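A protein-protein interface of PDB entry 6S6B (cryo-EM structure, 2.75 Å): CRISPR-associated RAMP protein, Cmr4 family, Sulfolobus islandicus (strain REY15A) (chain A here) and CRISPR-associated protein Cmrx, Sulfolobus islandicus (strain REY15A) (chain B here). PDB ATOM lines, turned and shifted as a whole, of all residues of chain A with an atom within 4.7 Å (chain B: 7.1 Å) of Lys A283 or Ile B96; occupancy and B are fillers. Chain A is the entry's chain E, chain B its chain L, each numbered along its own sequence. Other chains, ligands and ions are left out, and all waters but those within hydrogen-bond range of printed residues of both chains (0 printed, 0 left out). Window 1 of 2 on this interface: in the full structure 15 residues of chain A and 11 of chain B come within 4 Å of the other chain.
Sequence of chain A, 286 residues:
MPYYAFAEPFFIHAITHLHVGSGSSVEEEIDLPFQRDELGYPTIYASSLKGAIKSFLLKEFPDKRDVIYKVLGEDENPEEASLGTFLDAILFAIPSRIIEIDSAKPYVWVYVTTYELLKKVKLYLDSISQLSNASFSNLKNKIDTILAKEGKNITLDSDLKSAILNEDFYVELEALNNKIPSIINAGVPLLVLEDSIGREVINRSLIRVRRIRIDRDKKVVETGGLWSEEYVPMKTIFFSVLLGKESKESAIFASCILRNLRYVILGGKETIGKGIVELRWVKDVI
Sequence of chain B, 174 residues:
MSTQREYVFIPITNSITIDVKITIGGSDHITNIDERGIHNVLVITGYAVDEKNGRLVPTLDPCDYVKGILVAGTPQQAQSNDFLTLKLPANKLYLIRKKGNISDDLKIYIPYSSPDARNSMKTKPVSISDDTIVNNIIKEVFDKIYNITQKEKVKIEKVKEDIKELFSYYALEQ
The side-chain amino group (NZ) of Lys A283 is in salt-bridge range of the side-chain carboxylate (OE2) of Glu A8.
The backbone carbonyl oxygen (O) of Trp A281 sits close to the side-chain carboxylate (OD1) of Asp A284 (2.7 Å).
The backbone NH (N) of Asn B40 sits at hydrogen-bond distance from the backbone carbonyl oxygen (O) of Ile B96, at 3.1 Å.
The backbone NH (N) of Asn B40 is in hydrogen-bond range of the backbone carbonyl oxygen (O) of Arg B97, at 2.6 Å.
The backbone carbonyl oxygen (O) of Val B41 is in hydrogen-bond range of the backbone NH (N) of Ile B96, 2.6 Å away.
The backbone NH (N) of Val B43 lies within hydrogen-bond range of the backbone carbonyl oxygen (O) of Tyr B94.
Lys A283 touches just these residues of chain B: Tyr B94 (3.3 Å), Ile B96 (3.8 Å) and Arg B97 (3.8 Å).
Printed residues of chain B within 4 Å of Asp A284: Arg B97 (3.5 Å) and Lys B98 (3.96 Å).
Of the printed residues of chain A, Leu B95 touches Arg A259 (3.0 Å).
Printed residues of chain A within 4 Å of Ile B96: Arg A259 and Lys A283.
Of the printed residues of chain A, Arg B97 touches Lys A283 and Asp A284.
Printed residues of chain A within 4 Å of Lys B98: Asp A284.
The nearest residue of chain B that does not touch Lys A283 is Leu B166 (5.3 Å).
The nearest printed residue of chain A that does not touch Leu B95 is Asp A284 (5.7 Å).
The guanidinium group (NH2) of Arg A259 sits at hydrogen-bond distance from the backbone carbonyl oxygen (O) of Leu B95, at 3.0 Å.
The side-chain amino group (NZ) of Lys A283 is in hydrogen-bond range of the side-chain hydroxyl (OH) of Tyr B94 (3.3 Å).
Of the 16 printed residues of chain B, 5 touch a printed residue of chain A.
Hydrophobic or aromatic side chains of chain B that line the printed part of chain A: Tyr B94 and Ile B96.
Among the printed residues, 8 pairs touch across the chains.
Among the printed residues, no Asp or Glu carboxylate lies within 4 Å of a Lys or Arg side-chain nitrogen of the other chain.
Arg A259 touches Tyr B94 (CG to CE1, 3.3 Å).
Arg A259 touches Ile B96.
CD1 of Ile B96 touches CE of Lys A283, 3.8 Å away.
Lys A283 touches Arg B97.
Asp A284 touches Arg B97 (CB to N, 3.5 Å).
Lys B98 touches Asp A284.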
ATOM      1  N   GLU A   8      -6.874  23.329  40.063  1.00  0.00           N
ATOM      2  CA  GLU A   8      -8.194  22.992  39.537  1.00  0.00           C
ATOM      3  C   GLU A   8      -9.212  22.954  40.665  1.00  0.00           C
ATOM      4  O   GLU A   8      -9.474  21.886  41.236  1.00  0.00           O
ATOM      5  CB  GLU A   8      -8.156  21.654  38.805  1.00  0.00           C
ATOM      6  CG  GLU A   8      -7.272  21.647  37.582  1.00  0.00           C
ATOM      7  CD  GLU A   8      -7.630  22.747  36.598  1.00  0.00           C
ATOM      8  OE1 GLU A   8      -8.825  23.096  36.491  1.00  0.00           O
ATOM      9  OE2 GLU A   8      -6.713  23.267  35.926  1.00  0.00           O
ATOM     10  N   PRO A   9      -9.810  24.082  41.021  1.00  0.00           N
ATOM     11  CA  PRO A   9     -10.927  24.044  41.961  1.00  0.00           C
ATOM     12  C   PRO A   9     -12.120  23.361  41.328  1.00  0.00           C
ATOM     13  O   PRO A   9     -12.269  23.327  40.106  1.00  0.00           O
ATOM     14  CB  PRO A   9     -11.213  25.522  42.242  1.00  0.00           C
ATOM     15  CG  PRO A   9     -10.650  26.240  41.107  1.00  0.00           C
ATOM     16  CD  PRO A   9      -9.475  25.454  40.629  1.00  0.00           C
ATOM     17  N   ARG A 259     -10.389  15.330  33.275  1.00  0.00           N
ATOM     18  CA  ARG A 259     -11.501  15.591  32.378  1.00  0.00           C
ATOM     19  C   ARG A 259     -12.392  14.377  32.195  1.00  0.00           C
ATOM     20  O   ARG A 259     -13.476  14.502  31.620  1.00  0.00           O
ATOM     21  CB  ARG A 259     -10.982  16.060  31.021  1.00  0.00           C
ATOM     22  CG  ARG A 259      -9.793  16.979  31.132  1.00  0.00           C
ATOM     23  CD  ARG A 259     -10.139  18.260  31.864  1.00  0.00           C
ATOM     24  NE  ARG A 259     -10.973  19.142  31.058  1.00  0.00           N
ATOM     25  CZ  ARG A 259     -11.911  19.938  31.556  1.00  0.00           C
ATOM     26  NH1 ARG A 259     -12.135  19.958  32.861  1.00  0.00           N
ATOM     27  NH2 ARG A 259     -12.627  20.712  30.754  1.00  0.00           N
ATOM     28  N   TRP A 281     -15.887  20.667  37.675  1.00  0.00           N
ATOM     29  CA  TRP A 281     -14.712  21.522  37.702  1.00  0.00           C
ATOM     30  C   TRP A 281     -15.080  22.974  37.453  1.00  0.00           C
ATOM     31  O   TRP A 281     -15.906  23.285  36.597  1.00  0.00           O
ATOM     32  CB  TRP A 281     -13.709  21.039  36.666  1.00  0.00           C
ATOM     33  CG  TRP A 281     -13.410  19.612  36.859  1.00  0.00           C
ATOM     34  CD1 TRP A 281     -13.972  18.569  36.207  1.00  0.00           C
ATOM     35  CD2 TRP A 281     -12.501  19.055  37.806  1.00  0.00           C
ATOM     36  NE1 TRP A 281     -13.460  17.388  36.673  1.00  0.00           N
ATOM     37  CE2 TRP A 281     -12.553  17.662  37.659  1.00  0.00           C
ATOM     38  CE3 TRP A 281     -11.641  19.600  38.757  1.00  0.00           C
ATOM     39  CZ2 TRP A 281     -11.780  16.805  38.428  1.00  0.00           C
ATOM     40  CZ3 TRP A 281     -10.877  18.751  39.516  1.00  0.00           C
ATOM     41  CH2 TRP A 281     -10.950  17.369  39.350  1.00  0.00           C
ATOM     42  N   VAL A 282     -14.466  23.870  38.225  1.00  0.00           N
ATOM     43  CA  VAL A 282     -14.739  25.292  38.064  1.00  0.00           C
ATOM     44  C   VAL A 282     -14.306  25.768  36.688  1.00  0.00           C
ATOM     45  O   VAL A 282     -14.916  26.678  36.117  1.00  0.00           O
ATOM     46  CB  VAL A 282     -14.052  26.098  39.183  1.00  0.00           C
ATOM     47  CG1 VAL A 282     -14.271  27.579  38.986  1.00  0.00           C
ATOM     48  CG2 VAL A 282     -14.577  25.675  40.528  1.00  0.00           C
ATOM     49  N   LYS A 283     -13.267  25.154  36.122  1.00  0.00           N
ATOM     50  CA  LYS A 283     -12.753  25.616  34.839  1.00  0.00           C
ATOM     51  C   LYS A 283     -13.794  25.503  33.737  1.00  0.00           C
ATOM     52  O   LYS A 283     -13.736  26.251  32.756  1.00  0.00           O
ATOM     53  CB  LYS A 283     -11.498  24.834  34.462  1.00  0.00           C
ATOM     54  CG  LYS A 283     -11.775  23.511  33.790  1.00  0.00           C
ATOM     55  CD  LYS A 283     -10.532  22.654  33.744  1.00  0.00           C
ATOM     56  CE  LYS A 283      -9.418  23.337  32.976  1.00  0.00           C
ATOM     57  NZ  LYS A 283      -8.290  22.403  32.725  1.00  0.00           N
ATOM     58  N   ASP A 284     -14.753  24.586  33.874  1.00  0.00           N
ATOM     59  CA  ASP A 284     -15.807  24.436  32.879  1.00  0.00           C
ATOM     60  C   ASP A 284     -17.200  24.621  33.475  1.00  0.00           C
ATOM     61  O   ASP A 284     -18.179  24.125  32.913  1.00  0.00           O
ATOM     62  CB  ASP A 284     -15.692  23.083  32.169  1.00  0.00           C
ATOM     63  CG  ASP A 284     -15.764  21.899  33.112  1.00  0.00           C
ATOM     64  OD1 ASP A 284     -16.345  22.021  34.205  1.00  0.00           O
ATOM     65  OD2 ASP A 284     -15.241  20.826  32.745  1.00  0.00           O
ATOM     66  N   VAL A 285     -17.312  25.329  34.600  1.00  0.00           N
ATOM     67  CA  VAL A 285     -18.610  25.548  35.231  1.00  0.00           C
ATOM     68  C   VAL A 285     -19.225  26.878  34.828  1.00  0.00           C
ATOM     69  O   VAL A 285     -20.399  27.128  35.146  1.00  0.00           O
ATOM     70  CB  VAL A 285     -18.509  25.477  36.770  1.00  0.00           C
ATOM     71  CG1 VAL A 285     -17.924  26.767  37.325  1.00  0.00           C
ATOM     72  CG2 VAL A 285     -19.857  25.149  37.398  1.00  0.00           C
ATOM     73  N   THR B  31     -17.219  26.627  19.408  1.00  0.00           N
ATOM     74  CA  THR B  31     -17.090  27.639  20.444  1.00  0.00           C
ATOM     75  C   THR B  31     -18.100  28.746  20.201  1.00  0.00           C
ATOM     76  O   THR B  31     -18.028  29.459  19.198  1.00  0.00           O
ATOM     77  CB  THR B  31     -15.674  28.206  20.472  1.00  0.00           C
ATOM     78  OG1 THR B  31     -15.538  29.209  19.462  1.00  0.00           O
ATOM     79  CG2 THR B  31     -14.673  27.103  20.224  1.00  0.00           C
ATOM     80  N   ILE B  38     -16.953  32.510  26.032  1.00  0.00           N
ATOM     81  CA  ILE B  38     -16.651  31.484  25.044  1.00  0.00           C
ATOM     82  C   ILE B  38     -16.791  30.123  25.709  1.00  0.00           C
ATOM     83  O   ILE B  38     -16.377  29.940  26.857  1.00  0.00           O
ATOM     84  CB  ILE B  38     -15.245  31.673  24.446  1.00  0.00           C
ATOM     85  CG1 ILE B  38     -15.123  33.031  23.758  1.00  0.00           C
ATOM     86  CG2 ILE B  38     -14.942  30.579  23.440  1.00  0.00           C
ATOM     87  CD1 ILE B  38     -14.582  34.125  24.639  1.00  0.00           C
ATOM     88  N   HIS B  39     -17.369  29.160  24.996  1.00  0.00           N
ATOM     89  CA  HIS B  39     -17.507  27.805  25.504  1.00  0.00           C
ATOM     90  C   HIS B  39     -16.753  26.858  24.586  1.00  0.00           C
ATOM     91  O   HIS B  39     -16.318  27.244  23.501  1.00  0.00           O
ATOM     92  CB  HIS B  39     -18.971  27.366  25.588  1.00  0.00           C
ATOM     93  CG  HIS B  39     -19.797  28.183  26.529  1.00  0.00           C
ATOM     94  ND1 HIS B  39     -20.302  27.675  27.706  1.00  0.00           N
ATOM     95  CD2 HIS B  39     -20.219  29.466  26.461  1.00  0.00           C
ATOM     96  CE1 HIS B  39     -20.994  28.615  28.326  1.00  0.00           C
ATOM     97  NE2 HIS B  39     -20.959  29.711  27.591  1.00  0.00           N
ATOM     98  N   ASN B  40     -16.603  25.615  25.041  1.00  0.00           N
ATOM     99  CA  ASN B  40     -16.068  24.527  24.223  1.00  0.00           C
ATOM    100  C   ASN B  40     -14.755  24.908  23.546  1.00  0.00           C
ATOM    101  O   ASN B  40     -14.507  24.554  22.394  1.00  0.00           O
ATOM    102  CB  ASN B  40     -17.094  24.069  23.190  1.00  0.00           C
ATOM    103  CG  ASN B  40     -18.449  23.803  23.799  1.00  0.00           C
ATOM    104  OD1 ASN B  40     -18.675  22.757  24.407  1.00  0.00           O
ATOM    105  ND2 ASN B  40     -19.364  24.749  23.640  1.00  0.00           N
ATOM    106  N   VAL B  41     -13.911  25.647  24.262  1.00  0.00           N
ATOM    107  CA  VAL B  41     -12.592  25.987  23.745  1.00  0.00           C
ATOM    108  C   VAL B  41     -11.756  24.722  23.631  1.00  0.00           C
ATOM    109  O   VAL B  41     -11.845  23.823  24.475  1.00  0.00           O
ATOM    110  CB  VAL B  41     -11.910  27.019  24.653  1.00  0.00           C
ATOM    111  CG1 VAL B  41     -10.661  27.557  23.992  1.00  0.00           C
ATOM    112  CG2 VAL B  41     -12.865  28.137  24.981  1.00  0.00           C
ATOM    113  N   LEU B  42     -10.939  24.646  22.586  1.00  0.00           N
ATOM    114  CA  LEU B  42     -10.056  23.506  22.402  1.00  0.00           C
ATOM    115  C   LEU B  42      -8.675  23.794  22.972  1.00  0.00           C
ATOM    116  O   LEU B  42      -8.224  24.941  23.019  1.00  0.00           O
ATOM    117  CB  LEU B  42      -9.934  23.151  20.921  1.00  0.00           C
ATOM    118  CG  LEU B  42      -9.313  21.789  20.613  1.00  0.00           C
ATOM    119  CD1 LEU B  42     -10.001  20.708  21.411  1.00  0.00           C
ATOM    120  CD2 LEU B  42      -9.364  21.479  19.138  1.00  0.00           C
ATOM    121  N   VAL B  43      -8.004  22.734  23.417  1.00  0.00           N
ATOM    122  CA  VAL B  43      -6.611  22.809  23.839  1.00  0.00           C
ATOM    123  C   VAL B  43      -5.881  21.632  23.217  1.00  0.00           C
ATOM    124  O   VAL B  43      -6.329  20.488  23.338  1.00  0.00           O
ATOM    125  CB  VAL B  43      -6.448  22.778  25.366  1.00  0.00           C
ATOM    126  CG1 VAL B  43      -4.980  22.845  25.743  1.00  0.00           C
ATOM    127  CG2 VAL B  43      -7.242  23.883  26.024  1.00  0.00           C
ATOM    128  N   LYS B  67      -4.286  26.909  23.367  1.00  0.00           N
ATOM    129  CA  LYS B  67      -5.737  27.004  23.424  1.00  0.00           C
ATOM    130  C   LYS B  67      -6.243  27.871  22.279  1.00  0.00           C
ATOM    131  O   LYS B  67      -5.686  28.939  22.010  1.00  0.00           O
ATOM    132  CB  LYS B  67      -6.195  27.586  24.761  1.00  0.00           C
ATOM    133  CG  LYS B  67      -5.527  26.995  25.983  1.00  0.00           C
ATOM    134  CD  LYS B  67      -6.441  27.127  27.185  1.00  0.00           C
ATOM    135  CE  LYS B  67      -5.672  27.153  28.485  1.00  0.00           C
ATOM    136  NZ  LYS B  67      -5.225  28.527  28.825  1.00  0.00           N
ATOM    137  N   TYR B  94     -10.090  17.529  23.688  1.00  0.00           N
ATOM    138  CA  TYR B  94      -9.867  18.089  25.013  1.00  0.00           C
ATOM    139  C   TYR B  94     -10.477  19.486  24.995  1.00  0.00           C
ATOM    140  O   TYR B  94      -9.805  20.471  24.693  1.00  0.00           O
ATOM    141  CB  TYR B  94      -8.383  18.115  25.346  1.00  0.00           C
ATOM    142  CG  TYR B  94      -8.050  18.758  26.671  1.00  0.00           C
ATOM    143  CD1 TYR B  94      -8.189  18.076  27.862  1.00  0.00           C
ATOM    144  CD2 TYR B  94      -7.605  20.059  26.724  1.00  0.00           C
ATOM    145  CE1 TYR B  94      -7.878  18.684  29.064  1.00  0.00           C
ATOM    146  CE2 TYR B  94      -7.299  20.670  27.915  1.00  0.00           C
ATOM    147  CZ  TYR B  94      -7.436  19.983  29.082  1.00  0.00           C
ATOM    148  OH  TYR B  94      -7.125  20.604  30.269  1.00  0.00           O
ATOM    149  N   LEU B  95     -11.766  19.560  25.300  1.00  0.00           N
ATOM    150  CA  LEU B  95     -12.494  20.817  25.305  1.00  0.00           C
ATOM    151  C   LEU B  95     -12.500  21.429  26.697  1.00  0.00           C
ATOM    152  O   LEU B  95     -12.478  20.725  27.708  1.00  0.00           O
ATOM    153  CB  LEU B  95     -13.932  20.623  24.830  1.00  0.00           C
ATOM    154  CG  LEU B  95     -14.157  20.504  23.326  1.00  0.00           C
ATOM    155  CD1 LEU B  95     -15.627  20.662  23.012  1.00  0.00           C
ATOM    156  CD2 LEU B  95     -13.343  21.541  22.585  1.00  0.00           C
ATOM    157  N   ILE B  96     -12.539  22.756  26.736  1.00  0.00           N
ATOM    158  CA  ILE B  96     -12.629  23.514  27.974  1.00  0.00           C
ATOM    159  C   ILE B  96     -13.931  24.297  27.959  1.00  0.00           C
ATOM    160  O   ILE B  96     -14.322  24.848  26.926  1.00  0.00           O
ATOM    161  CB  ILE B  96     -11.422  24.455  28.155  1.00  0.00           C
ATOM    162  CG1 ILE B  96     -10.134  23.643  28.212  1.00  0.00           C
ATOM    163  CG2 ILE B  96     -11.569  25.280  29.407  1.00  0.00           C
ATOM    164  CD1 ILE B  96     -10.101  22.658  29.345  1.00  0.00           C
ATOM    165  N   ARG B  97     -14.604  24.331  29.105  1.00  0.00           N
ATOM    166  CA  ARG B  97     -15.877  25.023  29.260  1.00  0.00           C
ATOM    167  C   ARG B  97     -16.928  24.436  28.320  1.00  0.00           C
ATOM    168  O   ARG B  97     -17.489  25.112  27.458  1.00  0.00           O
ATOM    169  CB  ARG B  97     -15.706  26.528  29.054  1.00  0.00           C
ATOM    170  CG  ARG B  97     -16.832  27.348  29.630  1.00  0.00           C
ATOM    171  CD  ARG B  97     -16.457  28.808  29.734  1.00  0.00           C
ATOM    172  NE  ARG B  97     -15.483  29.044  30.790  1.00  0.00           N
ATOM    173  CZ  ARG B  97     -15.042  30.246  31.137  1.00  0.00           C
ATOM    174  NH1 ARG B  97     -15.488  31.323  30.509  1.00  0.00           N
ATOM    175  NH2 ARG B  97     -14.157  30.372  32.115  1.00  0.00           N
ATOM    176  N   LYS B  98     -17.172  23.142  28.501  1.00  0.00           N
ATOM    177  CA  LYS B  98     -18.193  22.436  27.743  1.00  0.00           C
ATOM    178  C   LYS B  98     -19.545  23.130  27.866  1.00  0.00           C
ATOM    179  O   LYS B  98     -19.884  23.698  28.906  1.00  0.00           O
ATOM    180  CB  LYS B  98     -18.330  21.002  28.249  1.00  0.00           C
ATOM    181  CG  LYS B  98     -17.121  20.112  28.052  1.00  0.00           C
ATOM    182  CD  LYS B  98     -17.109  19.489  26.672  1.00  0.00           C
ATOM    183  CE  LYS B  98     -16.031  18.425  26.571  1.00  0.00           C
ATOM    184  NZ  LYS B  98     -16.334  17.265  27.444  1.00  0.00           N
ATOM    185  N   LYS B  99     -20.315  23.094  26.780  1.00  0.00           N
ATOM    186  CA  LYS B  99     -21.725  23.459  26.818  1.00  0.00           C
ATOM    187  C   LYS B  99     -22.616  22.296  26.401  1.00  0.00           C
ATOM    188  O   LYS B  99     -23.552  21.942  27.123  1.00  0.00           O
ATOM    189  CB  LYS B  99     -21.992  24.681  25.932  1.00  0.00           C
ATOM    190  CG  LYS B  99     -23.329  25.347  26.206  1.00  0.00           C
ATOM    191  CD  LYS B  99     -23.795  26.172  25.021  1.00  0.00           C
ATOM    192  CE  LYS B  99     -22.826  27.295  24.707  1.00  0.00           C
ATOM    193  NZ  LYS B  99     -23.048  28.467  25.591  1.00  0.00           N
ATOM    194  N   GLU B 165      -8.375  35.327  30.626  1.00  0.00           N
ATOM    195  CA  GLU B 165      -8.327  34.217  31.565  1.00  0.00           C
ATOM    196  C   GLU B 165      -8.199  32.857  30.902  1.00  0.00           C
ATOM    197  O   GLU B 165      -7.470  32.007  31.413  1.00  0.00           O
ATOM    198  CB  GLU B 165      -9.574  34.214  32.457  1.00  0.00           C
ATOM    199  CG  GLU B 165      -9.556  33.134  33.529  1.00  0.00           C
ATOM    200  CD  GLU B 165     -10.746  33.204  34.467  1.00  0.00           C
ATOM    201  OE1 GLU B 165     -11.609  34.081  34.275  1.00  0.00           O
ATOM    202  OE2 GLU B 165     -10.817  32.381  35.402  1.00  0.00           O
ATOM    203  N   LEU B 166      -8.873  32.630  29.778  1.00  0.00           N
ATOM    204  CA  LEU B 166      -8.889  31.303  29.171  1.00  0.00           C
ATOM    205  C   LEU B 166      -7.596  30.989  28.429  1.00  0.00           C
ATOM    206  O   LEU B 166      -6.891  30.039  28.779  1.00  0.00           O
ATOM    207  CB  LEU B 166     -10.092  31.166  28.236  1.00  0.00           C
ATOM    208  CG  LEU B 166     -11.349  30.561  28.857  1.00  0.00           C
ATOM    209  CD1 LEU B 166     -11.124  29.089  29.151  1.00  0.00           C
ATOM    210  CD2 LEU B 166     -11.720  31.288  30.130  1.00  0.00           C
